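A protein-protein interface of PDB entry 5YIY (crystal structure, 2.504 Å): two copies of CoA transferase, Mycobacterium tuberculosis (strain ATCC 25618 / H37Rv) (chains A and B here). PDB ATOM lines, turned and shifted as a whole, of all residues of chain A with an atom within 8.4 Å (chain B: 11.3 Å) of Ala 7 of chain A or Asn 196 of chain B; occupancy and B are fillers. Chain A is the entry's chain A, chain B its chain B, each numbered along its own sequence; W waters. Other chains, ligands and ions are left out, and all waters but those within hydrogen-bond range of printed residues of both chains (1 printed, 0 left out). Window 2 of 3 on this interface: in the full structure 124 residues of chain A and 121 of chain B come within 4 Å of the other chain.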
ATOM      1  N   ASN A   5     -18.990  11.990 -33.187  1.00  0.00           N
ATOM      2  CA  ASN A   5     -19.870  11.713 -32.071  1.00  0.00           C
ATOM      3  C   ASN A   5     -19.127  11.915 -30.782  1.00  0.00           C
ATOM      4  O   ASN A   5     -18.145  11.262 -30.521  1.00  0.00           O
ATOM      5  CB  ASN A   5     -20.393  10.304 -32.144  1.00  0.00           C
ATOM      6  N   PRO A   6     -19.590  12.848 -29.976  1.00  0.00           N
ATOM      7  CA  PRO A   6     -18.981  13.133 -28.690  1.00  0.00           C
ATOM      8  C   PRO A   6     -19.287  12.058 -27.704  1.00  0.00           C
ATOM      9  O   PRO A   6     -20.263  11.359 -27.829  1.00  0.00           O
ATOM     10  CB  PRO A   6     -19.616  14.443 -28.269  1.00  0.00           C
ATOM     11  CG  PRO A   6     -20.785  14.620 -29.120  1.00  0.00           C
ATOM     12  CD  PRO A   6     -20.611  13.821 -30.351  1.00  0.00           C
ATOM     13  N   ALA A   7     -18.439  11.943 -26.713  1.00  0.00           N
ATOM     14  CA  ALA A   7     -18.586  10.952 -25.685  1.00  0.00           C
ATOM     15  C   ALA A   7     -19.815  11.154 -24.809  1.00  0.00           C
ATOM     16  O   ALA A   7     -20.296  12.242 -24.654  1.00  0.00           O
ATOM     17  CB  ALA A   7     -17.349  10.939 -24.830  1.00  0.00           C
ATOM     18  N   LYS A   8     -20.328  10.070 -24.264  1.00  0.00           N
ATOM     19  CA  LYS A   8     -21.478  10.099 -23.402  1.00  0.00           C
ATOM     20  C   LYS A   8     -21.131   9.418 -22.099  1.00  0.00           C
ATOM     21  O   LYS A   8     -20.306   8.556 -22.048  1.00  0.00           O
ATOM     22  CB  LYS A   8     -22.649   9.416 -24.056  1.00  0.00           C
ATOM     23  CG  LYS A   8     -23.196  10.121 -25.266  1.00  0.00           C
ATOM     24  CD  LYS A   8     -24.566   9.584 -25.602  1.00  0.00           C
ATOM     25  CE  LYS A   8     -25.142  10.243 -26.827  1.00  0.00           C
ATOM     26  NZ  LYS A   8     -26.437   9.644 -27.188  1.00  0.00           N
ATOM     27  N   PRO A   9     -21.841   9.758 -21.049  1.00  0.00           N
ATOM     28  CA  PRO A   9     -21.525   9.302 -19.715  1.00  0.00           C
ATOM     29  C   PRO A   9     -21.456   7.825 -19.539  1.00  0.00           C
ATOM     30  O   PRO A   9     -20.716   7.392 -18.710  1.00  0.00           O
ATOM     31  CB  PRO A   9     -22.666   9.863 -18.913  1.00  0.00           C
ATOM     32  CG  PRO A   9     -22.967  11.126 -19.586  1.00  0.00           C
ATOM     33  CD  PRO A   9     -22.849  10.817 -21.026  1.00  0.00           C
ATOM     34  N   LEU A  10     -22.256   7.067 -20.244  1.00  0.00           N
ATOM     35  CA  LEU A  10     -22.256   5.629 -20.090  1.00  0.00           C
ATOM     36  C   LEU A  10     -21.610   4.835 -21.201  1.00  0.00           C
ATOM     37  O   LEU A  10     -21.860   3.678 -21.322  1.00  0.00           O
ATOM     38  CB  LEU A  10     -23.659   5.131 -19.839  1.00  0.00           C
ATOM     39  CG  LEU A  10     -24.372   5.933 -18.783  1.00  0.00           C
ATOM     40  CD1 LEU A  10     -25.732   5.378 -18.487  1.00  0.00           C
ATOM     41  CD2 LEU A  10     -23.558   6.065 -17.526  1.00  0.00           C
ATOM     42  N   ASP A  11     -20.804   5.459 -22.031  1.00  0.00           N
ATOM     43  CA  ASP A  11     -20.159   4.731 -23.103  1.00  0.00           C
ATOM     44  C   ASP A  11     -19.291   3.632 -22.523  1.00  0.00           C
ATOM     45  O   ASP A  11     -18.434   3.873 -21.729  1.00  0.00           O
ATOM     46  CB  ASP A  11     -19.265   5.670 -23.893  1.00  0.00           C
ATOM     47  CG  ASP A  11     -19.998   6.464 -24.915  1.00  0.00           C
ATOM     48  OD1 ASP A  11     -21.068   6.056 -25.371  1.00  0.00           O
ATOM     49  OD2 ASP A  11     -19.471   7.510 -25.285  1.00  0.00           O
ATOM     50  N   GLY A  12     -19.472   2.430 -23.029  1.00  0.00           N
ATOM     51  CA  GLY A  12     -18.764   1.256 -22.584  1.00  0.00           C
ATOM     52  C   GLY A  12     -19.416   0.399 -21.533  1.00  0.00           C
ATOM     53  O   GLY A  12     -18.950  -0.684 -21.253  1.00  0.00           O
ATOM     54  N   ASP A  33     -30.015   6.603 -23.898  1.00  0.00           N
ATOM     55  CA  ASP A  33     -29.792   7.987 -24.298  1.00  0.00           C
ATOM     56  C   ASP A  33     -28.487   8.528 -23.721  1.00  0.00           C
ATOM     57  O   ASP A  33     -27.864   9.421 -24.299  1.00  0.00           O
ATOM     58  CB  ASP A  33     -30.966   8.867 -23.862  1.00  0.00           C
ATOM     59  CG  ASP A  33     -32.232   8.581 -24.645  1.00  0.00           C
ATOM     60  OD1 ASP A  33     -32.154   7.862 -25.665  1.00  0.00           O
ATOM     61  OD2 ASP A  33     -33.306   9.074 -24.242  1.00  0.00           O
ATOM     62  N   LEU A  34     -28.075   7.982 -22.580  1.00  0.00           N
ATOM     63  CA  LEU A  34     -26.825   8.389 -21.948  1.00  0.00           C
ATOM     64  C   LEU A  34     -25.633   7.582 -22.464  1.00  0.00           C
ATOM     65  O   LEU A  34     -24.519   7.722 -21.961  1.00  0.00           O
ATOM     66  CB  LEU A  34     -26.929   8.262 -20.427  1.00  0.00           C
ATOM     67  CG  LEU A  34     -27.965   9.163 -19.752  1.00  0.00           C
ATOM     68  CD1 LEU A  34     -28.054   8.866 -18.262  1.00  0.00           C
ATOM     69  CD2 LEU A  34     -27.642  10.631 -19.993  1.00  0.00           C
ATOM     70  N   GLY A  35     -25.873   6.737 -23.462  1.00  0.00           N
ATOM     71  CA  GLY A  35     -24.795   6.065 -24.165  1.00  0.00           C
ATOM     72  C   GLY A  35     -24.518   4.620 -23.788  1.00  0.00           C
ATOM     73  O   GLY A  35     -23.608   4.001 -24.336  1.00  0.00           O
ATOM     74  N   GLU A 194     -17.566   3.690  -9.176  1.00  0.00           N
ATOM     75  CA  GLU A 194     -16.389   4.389  -9.683  1.00  0.00           C
ATOM     76  C   GLU A 194     -15.557   5.001  -8.558  1.00  0.00           C
ATOM     77  O   GLU A 194     -14.332   4.883  -8.547  1.00  0.00           O
ATOM     78  CB  GLU A 194     -16.801   5.479 -10.675  1.00  0.00           C
ATOM     79  CG  GLU A 194     -17.155   4.960 -12.059  1.00  0.00           C
ATOM     80  CD  GLU A 194     -15.937   4.500 -12.837  1.00  0.00           C
ATOM     81  OE1 GLU A 194     -16.073   3.573 -13.665  1.00  0.00           O
ATOM     82  OE2 GLU A 194     -14.844   5.069 -12.627  1.00  0.00           O
ATOM     83  N   TYR A 369     -28.379  18.049 -22.008  1.00  0.00           N
ATOM     84  CA  TYR A 369     -26.982  18.278 -21.680  1.00  0.00           C
ATOM     85  C   TYR A 369     -26.316  19.045 -22.816  1.00  0.00           C
ATOM     86  O   TYR A 369     -26.673  18.883 -23.985  1.00  0.00           O
ATOM     87  CB  TYR A 369     -26.254  16.949 -21.436  1.00  0.00           C
ATOM     88  CG  TYR A 369     -26.967  16.026 -20.465  1.00  0.00           C
ATOM     89  CD1 TYR A 369     -28.056  15.262 -20.873  1.00  0.00           C
ATOM     90  CD2 TYR A 369     -26.552  15.917 -19.142  1.00  0.00           C
ATOM     91  CE1 TYR A 369     -28.712  14.421 -19.997  1.00  0.00           C
ATOM     92  CE2 TYR A 369     -27.204  15.074 -18.258  1.00  0.00           C
ATOM     93  CZ  TYR A 369     -28.282  14.331 -18.693  1.00  0.00           C
ATOM     94  OH  TYR A 369     -28.934  13.490 -17.823  1.00  0.00           O
ATOM     95  N   SER A 371     -22.900  19.110 -23.639  1.00  0.00           N
ATOM     96  CA  SER A 371     -21.736  18.490 -24.262  1.00  0.00           C
ATOM     97  C   SER A 371     -22.083  17.276 -25.115  1.00  0.00           C
ATOM     98  O   SER A 371     -21.214  16.777 -25.841  1.00  0.00           O
ATOM     99  CB  SER A 371     -20.721  18.075 -23.192  1.00  0.00           C
ATOM    100  OG  SER A 371     -21.072  16.828 -22.621  1.00  0.00           O
ATOM    101  N   PHE A 372     -23.313  16.785 -25.041  1.00  0.00           N
ATOM    102  CA  PHE A 372     -23.752  15.677 -25.879  1.00  0.00           C
ATOM    103  C   PHE A 372     -25.266  15.764 -26.029  1.00  0.00           C
ATOM    104  O   PHE A 372     -25.921  16.620 -25.430  1.00  0.00           O
ATOM    105  CB  PHE A 372     -23.322  14.329 -25.295  1.00  0.00           C
ATOM    106  CG  PHE A 372     -24.011  13.977 -24.009  1.00  0.00           C
ATOM    107  CD1 PHE A 372     -23.558  14.478 -22.801  1.00  0.00           C
ATOM    108  CD2 PHE A 372     -25.119  13.146 -24.012  1.00  0.00           C
ATOM    109  CE1 PHE A 372     -24.197  14.156 -21.620  1.00  0.00           C
ATOM    110  CE2 PHE A 372     -25.759  12.821 -22.834  1.00  0.00           C
ATOM    111  CZ  PHE A 372     -25.299  13.325 -21.637  1.00  0.00           C
ATOM    112  N   ARG A 373     -25.819  14.849 -26.823  1.00  0.00           N
ATOM    113  CA  ARG A 373     -27.231  14.837 -27.202  1.00  0.00           C
ATOM    114  C   ARG A 373     -27.872  13.587 -26.610  1.00  0.00           C
ATOM    115  O   ARG A 373     -27.597  12.472 -27.066  1.00  0.00           O
ATOM    116  CB  ARG A 373     -27.355  14.856 -28.724  1.00  0.00           C
ATOM    117  CG  ARG A 373     -28.677  15.284 -29.308  1.00  0.00           C
ATOM    118  CD  ARG A 373     -28.477  15.410 -30.806  1.00  0.00           C
ATOM    119  NE  ARG A 373     -29.705  15.726 -31.517  1.00  0.00           N
ATOM    120  CZ  ARG A 373     -30.184  16.955 -31.649  1.00  0.00           C
ATOM    121  NH1 ARG A 373     -29.538  17.980 -31.103  1.00  0.00           N
ATOM    122  NH2 ARG A 373     -31.309  17.158 -32.321  1.00  0.00           N
ATOM    123  N   PRO B 123     -13.276  25.183 -14.083  1.00  0.00           N
ATOM    124  CA  PRO B 123     -13.413  24.243 -15.199  1.00  0.00           C
ATOM    125  C   PRO B 123     -13.935  22.884 -14.741  1.00  0.00           C
ATOM    126  O   PRO B 123     -14.211  22.015 -15.569  1.00  0.00           O
ATOM    127  CB  PRO B 123     -11.985  24.131 -15.729  1.00  0.00           C
ATOM    128  CG  PRO B 123     -11.140  24.319 -14.514  1.00  0.00           C
ATOM    129  CD  PRO B 123     -11.878  25.296 -13.628  1.00  0.00           C
ATOM    130  N   ASN B 124     -14.066  22.711 -13.430  1.00  0.00           N
ATOM    131  CA  ASN B 124     -14.567  21.466 -12.862  1.00  0.00           C
ATOM    132  C   ASN B 124     -16.031  21.577 -12.454  1.00  0.00           C
ATOM    133  O   ASN B 124     -16.629  20.611 -11.980  1.00  0.00           O
ATOM    134  CB  ASN B 124     -13.728  21.059 -11.650  1.00  0.00           C
ATOM    135  CG  ASN B 124     -12.384  20.479 -12.038  1.00  0.00           C
ATOM    136  OD1 ASN B 124     -12.063  20.361 -13.221  1.00  0.00           O
ATOM    137  ND2 ASN B 124     -11.586  20.116 -11.040  1.00  0.00           N
ATOM    138  N   ILE B 126     -19.967  21.755 -12.551  1.00  0.00           N
ATOM    139  CA  ILE B 126     -21.140  21.321 -13.296  1.00  0.00           C
ATOM    140  C   ILE B 126     -22.286  22.293 -13.043  1.00  0.00           C
ATOM    141  O   ILE B 126     -22.663  22.536 -11.897  1.00  0.00           O
ATOM    142  CB  ILE B 126     -21.568  19.895 -12.909  1.00  0.00           C
ATOM    143  CG1 ILE B 126     -20.512  18.885 -13.362  1.00  0.00           C
ATOM    144  CG2 ILE B 126     -22.918  19.560 -13.519  1.00  0.00           C
ATOM    145  CD1 ILE B 126     -20.700  17.505 -12.783  1.00  0.00           C
ATOM    146  N   LEU B 187     -26.416  13.576 -11.449  1.00  0.00           N
ATOM    147  CA  LEU B 187     -25.650  12.350 -11.250  1.00  0.00           C
ATOM    148  C   LEU B 187     -25.009  11.891 -12.556  1.00  0.00           C
ATOM    149  O   LEU B 187     -23.880  11.399 -12.564  1.00  0.00           O
ATOM    150  CB  LEU B 187     -26.542  11.243 -10.684  1.00  0.00           C
ATOM    151  CG  LEU B 187     -27.041  11.436  -9.251  1.00  0.00           C
ATOM    152  CD1 LEU B 187     -28.173  10.469  -8.941  1.00  0.00           C
ATOM    153  CD2 LEU B 187     -25.902  11.266  -8.258  1.00  0.00           C
ATOM    154  N   ALA B 188     -25.737  12.057 -13.654  1.00  0.00           N
ATOM    155  CA  ALA B 188     -25.222  11.725 -14.978  1.00  0.00           C
ATOM    156  C   ALA B 188     -24.036  12.614 -15.340  1.00  0.00           C
ATOM    157  O   ALA B 188     -23.044  12.145 -15.900  1.00  0.00           O
ATOM    158  CB  ALA B 188     -26.320  11.854 -16.022  1.00  0.00           C
ATOM    159  N   ALA B 189     -24.148  13.898 -15.016  1.00  0.00           N
ATOM    160  CA  ALA B 189     -23.090  14.862 -15.295  1.00  0.00           C
ATOM    161  C   ALA B 189     -21.831  14.549 -14.492  1.00  0.00           C
ATOM    162  O   ALA B 189     -20.714  14.707 -14.986  1.00  0.00           O
ATOM    163  CB  ALA B 189     -23.569  16.273 -15.001  1.00  0.00           C
ATOM    164  N   LEU B 190     -22.021  14.107 -13.252  1.00  0.00           N
ATOM    165  CA  LEU B 190     -20.903  13.734 -12.391  1.00  0.00           C
ATOM    166  C   LEU B 190     -20.171  12.518 -12.949  1.00  0.00           C
ATOM    167  O   LEU B 190     -18.943  12.444 -12.894  1.00  0.00           O
ATOM    168  CB  LEU B 190     -21.394  13.454 -10.969  1.00  0.00           C
ATOM    169  CG  LEU B 190     -21.890  14.664 -10.173  1.00  0.00           C
ATOM    170  CD1 LEU B 190     -22.712  14.219  -8.975  1.00  0.00           C
ATOM    171  CD2 LEU B 190     -20.718  15.522  -9.727  1.00  0.00           C
ATOM    172  N   LEU B 191     -20.932  11.567 -13.480  1.00  0.00           N
ATOM    173  CA  LEU B 191     -20.352  10.411 -14.155  1.00  0.00           C
ATOM    174  C   LEU B 191     -19.603  10.843 -15.408  1.00  0.00           C
ATOM    175  O   LEU B 191     -18.520  10.335 -15.704  1.00  0.00           O
ATOM    176  CB  LEU B 191     -21.436   9.392 -14.516  1.00  0.00           C
ATOM    177  CG  LEU B 191     -21.659   8.249 -13.526  1.00  0.00           C
ATOM    178  CD1 LEU B 191     -22.943   7.504 -13.851  1.00  0.00           C
ATOM    179  CD2 LEU B 191     -20.471   7.298 -13.530  1.00  0.00           C
ATOM    180  N   HIS B 192     -20.194  11.780 -16.144  1.00  0.00           N
ATOM    181  CA  HIS B 192     -19.592  12.305 -17.363  1.00  0.00           C
ATOM    182  C   HIS B 192     -18.259  12.979 -17.057  1.00  0.00           C
ATOM    183  O   HIS B 192     -17.295  12.842 -17.809  1.00  0.00           O
ATOM    184  CB  HIS B 192     -20.542  13.289 -18.048  1.00  0.00           C
ATOM    185  CG  HIS B 192     -20.212  13.550 -19.484  1.00  0.00           C
ATOM    186  ND1 HIS B 192     -19.737  12.569 -20.329  1.00  0.00           N
ATOM    187  CD2 HIS B 192     -20.294  14.678 -20.230  1.00  0.00           C
ATOM    188  CE1 HIS B 192     -19.538  13.081 -21.529  1.00  0.00           C
ATOM    189  NE2 HIS B 192     -19.868  14.361 -21.496  1.00  0.00           N
ATOM    190  N   ARG B 193     -18.217  13.706 -15.944  1.00  0.00           N
ATOM    191  CA  ARG B 193     -16.997  14.376 -15.511  1.00  0.00           C
ATOM    192  C   ARG B 193     -15.952  13.369 -15.048  1.00  0.00           C
ATOM    193  O   ARG B 193     -14.766  13.505 -15.346  1.00  0.00           O
ATOM    194  CB  ARG B 193     -17.297  15.367 -14.384  1.00  0.00           C
ATOM    195  CG  ARG B 193     -16.246  16.454 -14.222  1.00  0.00           C
ATOM    196  CD  ARG B 193     -16.568  17.375 -13.054  1.00  0.00           C
ATOM    197  NE  ARG B 193     -16.688  16.640 -11.798  1.00  0.00           N
ATOM    198  CZ  ARG B 193     -16.791  17.213 -10.604  1.00  0.00           C
ATOM    199  NH1 ARG B 193     -16.789  18.535 -10.498  1.00  0.00           N
ATOM    200  NH2 ARG B 193     -16.896  16.466  -9.513  1.00  0.00           N
ATOM    201  N   GLU B 194     -16.400  12.361 -14.308  1.00  0.00           N
ATOM    202  CA  GLU B 194     -15.504  11.343 -13.778  1.00  0.00           C
ATOM    203  C   GLU B 194     -14.878  10.495 -14.886  1.00  0.00           C
ATOM    204  O   GLU B 194     -13.674  10.242 -14.880  1.00  0.00           O
ATOM    205  CB  GLU B 194     -16.250  10.442 -12.791  1.00  0.00           C
ATOM    206  CG  GLU B 194     -15.393   9.945 -11.640  1.00  0.00           C
ATOM    207  CD  GLU B 194     -14.988  11.059 -10.695  1.00  0.00           C
ATOM    208  OE1 GLU B 194     -13.782  11.379 -10.630  1.00  0.00           O
ATOM    209  OE2 GLU B 194     -15.876  11.616 -10.015  1.00  0.00           O
ATOM    210  N   ARG B 195     -15.703  10.063 -15.835  1.00  0.00           N
ATOM    211  CA  ARG B 195     -15.257   9.140 -16.874  1.00  0.00           C
ATOM    212  C   ARG B 195     -14.658   9.834 -18.096  1.00  0.00           C
ATOM    213  O   ARG B 195     -13.664   9.369 -18.652  1.00  0.00           O
ATOM    214  CB  ARG B 195     -16.418   8.244 -17.313  1.00  0.00           C
ATOM    215  CG  ARG B 195     -16.988   7.386 -16.197  1.00  0.00           C
ATOM    216  CD  ARG B 195     -17.973   6.359 -16.730  1.00  0.00           C
ATOM    217  NE  ARG B 195     -17.293   5.191 -17.284  1.00  0.00           N
ATOM    218  CZ  ARG B 195     -17.425   4.772 -18.539  1.00  0.00           C
ATOM    219  NH1 ARG B 195     -18.218   5.426 -19.379  1.00  0.00           N
ATOM    220  NH2 ARG B 195     -16.768   3.698 -18.955  1.00  0.00           N
ATOM    221  N   ASN B 196     -15.260  10.943 -18.516  1.00  0.00           N
ATOM    222  CA  ASN B 196     -14.835  11.611 -19.744  1.00  0.00           C
ATOM    223  C   ASN B 196     -14.188  12.976 -19.520  1.00  0.00           C
ATOM    224  O   ASN B 196     -13.806  13.651 -20.476  1.00  0.00           O
ATOM    225  CB  ASN B 196     -16.026  11.758 -20.694  1.00  0.00           C
ATOM    226  CG  ASN B 196     -16.603  10.421 -21.117  1.00  0.00           C
ATOM    227  OD1 ASN B 196     -15.880   9.537 -21.576  1.00  0.00           O
ATOM    228  ND2 ASN B 196     -17.912  10.265 -20.961  1.00  0.00           N
ATOM    229  N   GLY B 197     -14.060  13.378 -18.259  1.00  0.00           N
ATOM    230  CA  GLY B 197     -13.418  14.637 -17.923  1.00  0.00           C
ATOM    231  C   GLY B 197     -14.142  15.864 -18.445  1.00  0.00           C
ATOM    232  O   GLY B 197     -13.513  16.871 -18.769  1.00  0.00           O
ATOM    233  N   VAL B 198     -15.465  15.782 -18.529  1.00  0.00           N
ATOM    234  CA  VAL B 198     -16.263  16.898 -19.020  1.00  0.00           C
ATOM    235  C   VAL B 198     -17.193  17.457 -17.947  1.00  0.00           C
ATOM    236  O   VAL B 198     -18.032  16.741 -17.403  1.00  0.00           O
ATOM    237  CB  VAL B 198     -17.111  16.487 -20.241  1.00  0.00           C
ATOM    238  CG1 VAL B 198     -18.021  17.629 -20.668  1.00  0.00           C
ATOM    239  CG2 VAL B 198     -16.214  16.053 -21.389  1.00  0.00           C
ATOM    240  N   ALA B 199     -17.044  18.745 -17.656  1.00  0.00           N
ATOM    241  CA  ALA B 199     -17.938  19.426 -16.727  1.00  0.00           C
ATOM    242  C   ALA B 199     -19.019  20.130 -17.534  1.00  0.00           C
ATOM    243  O   ALA B 199     -18.766  21.148 -18.177  1.00  0.00           O
ATOM    244  CB  ALA B 199     -17.175  20.412 -15.860  1.00  0.00           C
ATOM    245  N   ASP B 200     -20.228  19.583 -17.489  1.00  0.00           N
ATOM    246  CA  ASP B 200     -21.276  19.969 -18.425  1.00  0.00           C
ATOM    247  C   ASP B 200     -22.250  20.998 -17.866  1.00  0.00           C
ATOM    248  O   ASP B 200     -22.275  21.273 -16.667  1.00  0.00           O
ATOM    249  CB  ASP B 200     -22.052  18.728 -18.872  1.00  0.00           C
ATOM    250  CG  ASP B 200     -22.574  18.847 -20.289  1.00  0.00           C
ATOM    251  OD1 ASP B 200     -22.523  19.961 -20.851  1.00  0.00           O
ATOM    252  OD2 ASP B 200     -23.037  17.826 -20.841  1.00  0.00           O
HETATM  253  O   HOH W   1     -19.613  15.122 -24.479  1.00  0.00           O
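O of Ala 7 of chain A touches CE1 of His 192 of chain B, at 3.3 Å. Ala 188 of chain B touches Pro 9 of chain A. Pro 9 of chain A touches His 192 of chain B (N to ND1, 3.6 Å). Pro 9 of chain A touches Asn 196 of chain B (CA to ND2, 3.9 Å). CD1 of Leu 191 of chain B touches CD2 of Leu 10 of chain A, at 3.99 Å. Leu 10 of chain A touches Arg 195 of chain B. Tyr 369 of chain A touches Ala 188 of chain B (OH to CB, 3.6 Å). Asp 200 of chain B touches Tyr 369 of chain A (OD2 to CB, 3.4 Å). NE2 of His 192 of chain B touches CD1 of Phe 372 of chain A, 3.9 Å away. Phe 372 of chain A touches Asp 200 of chain B (CD1 to OD2, 3.9 Å).
The backbone carbonyl oxygen of His 192 of chain B sits at hydrogen-bond distance from the backbone NH of Gly 197 of chain B, at 3.3 Å. O of Leu 34 of chain A sits at hydrogen-bond distance from N of Leu 10 of chain A (2.9 Å). The side-chain amino group (NZ) of Lys 8 of chain A lies within hydrogen-bond range of the backbone carbonyl oxygen (O) of Asp 33 of chain A (3.2 Å). The side-chain amide nitrogen of Asn 196 of chain B sits at hydrogen-bond distance from a ring nitrogen (ND1) of His 192 of chain B. The backbone NH of Arg 193 of chain B lies close to the backbone carbonyl oxygen of Val 198 of chain B (3.4 Å). The backbone NH (N) of Lys 8 of chain A sits at hydrogen-bond distance from the side-chain carboxylate (OD2) of Asp 11 of chain A, at 2.9 Å.
O of Asp 11 of chain A sits at hydrogen-bond distance from NH1 of Arg 195 of chain B, 2.8 Å away. O of Pro 9 of chain A is in hydrogen-bond range of NH1 of Arg 195 of chain B (3.2 Å). A ring nitrogen (NE2) of His 192 of chain B is in hydrogen-bond range of the side-chain hydroxyl (OG) of Ser 371 of chain A. The side-chain amide nitrogen (ND2) of Asn 196 of chain B sits at hydrogen-bond distance from the backbone carbonyl oxygen (O) of Lys 8 of chain A (3.1 Å). The side-chain carboxylate of Asp 200 of chain B is in hydrogen-bond range of the side-chain hydroxyl of Ser 371 of chain A, 2.8 Å away.
Water W1 lies within hydrogen-bond range of the backbone carbonyl oxygen of Ser 371 of chain A (2.7 Å), the backbone carbonyl oxygen of Ala 7 of chain A (3.0 Å) and a ring nitrogen (NE2) of His 192 of chain B (3.1 Å).
Ala 7 of chain A touches just these residues of chain B: His 192 and Asn 196. Of chain A, only Ala 7 (3.8 Å), Lys 8 (3.1 Å) and Pro 9 (3.9 Å) come within 4 Å of Asn 196 of chain B. No residue of chain B comes within 4 Å of Asn 5 of chain A. Lys 8 of chain A touches just these residues of chain B: His 192 and Asn 196. Of the printed residues of chain B, Phe 372 of chain A touches His 192 (3.9 Å) and Asp 200 (3.9 Å). Of the printed residues of chain B, Leu 10 of chain A touches Leu 191 and Arg 195. Printed residues of chain A within 4 Å of Ala 188 of chain B: Pro 9 (3.8 Å) and Tyr 369 (3.6 Å). Printed residues of chain A within 4 Å of Asp 200 of chain B: Tyr 369, Ser 371 and Phe 372. Of the printed residues of chain B, Tyr 369 of chain A touches Ala 188 and Asp 200. Printed residues of chain A within 4 Å of Val 198 of chain B: Ser 371. Glu 194 of chain A touches none of the printed residues of chain B. The nearest residue of chain B that does not touch Ala 7 of chain A is Val 198 of chain B (6.3 Å). The nearest printed residue of chain A that does not touch Asp 200 of chain B is Pro 9 of chain A (6.8 Å).
1 position is printed for both chains.
Of the 16 printed residues of chain A, 8 touch a printed residue of chain B. Hydrophobic or aromatic side chains of chain A that line the printed part of chain B: Ala 7, Pro 9, Leu 10, Tyr 369 and Phe 372. Of the 17 printed residues of chain B, 7 touch a printed residue of chain A. Hydrophobic or aromatic side chains of chain B that line the printed part of chain A: Ala 188, Leu 191, His 192 and Val 198. Among the printed residues, 18 pairs touch across the chains.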
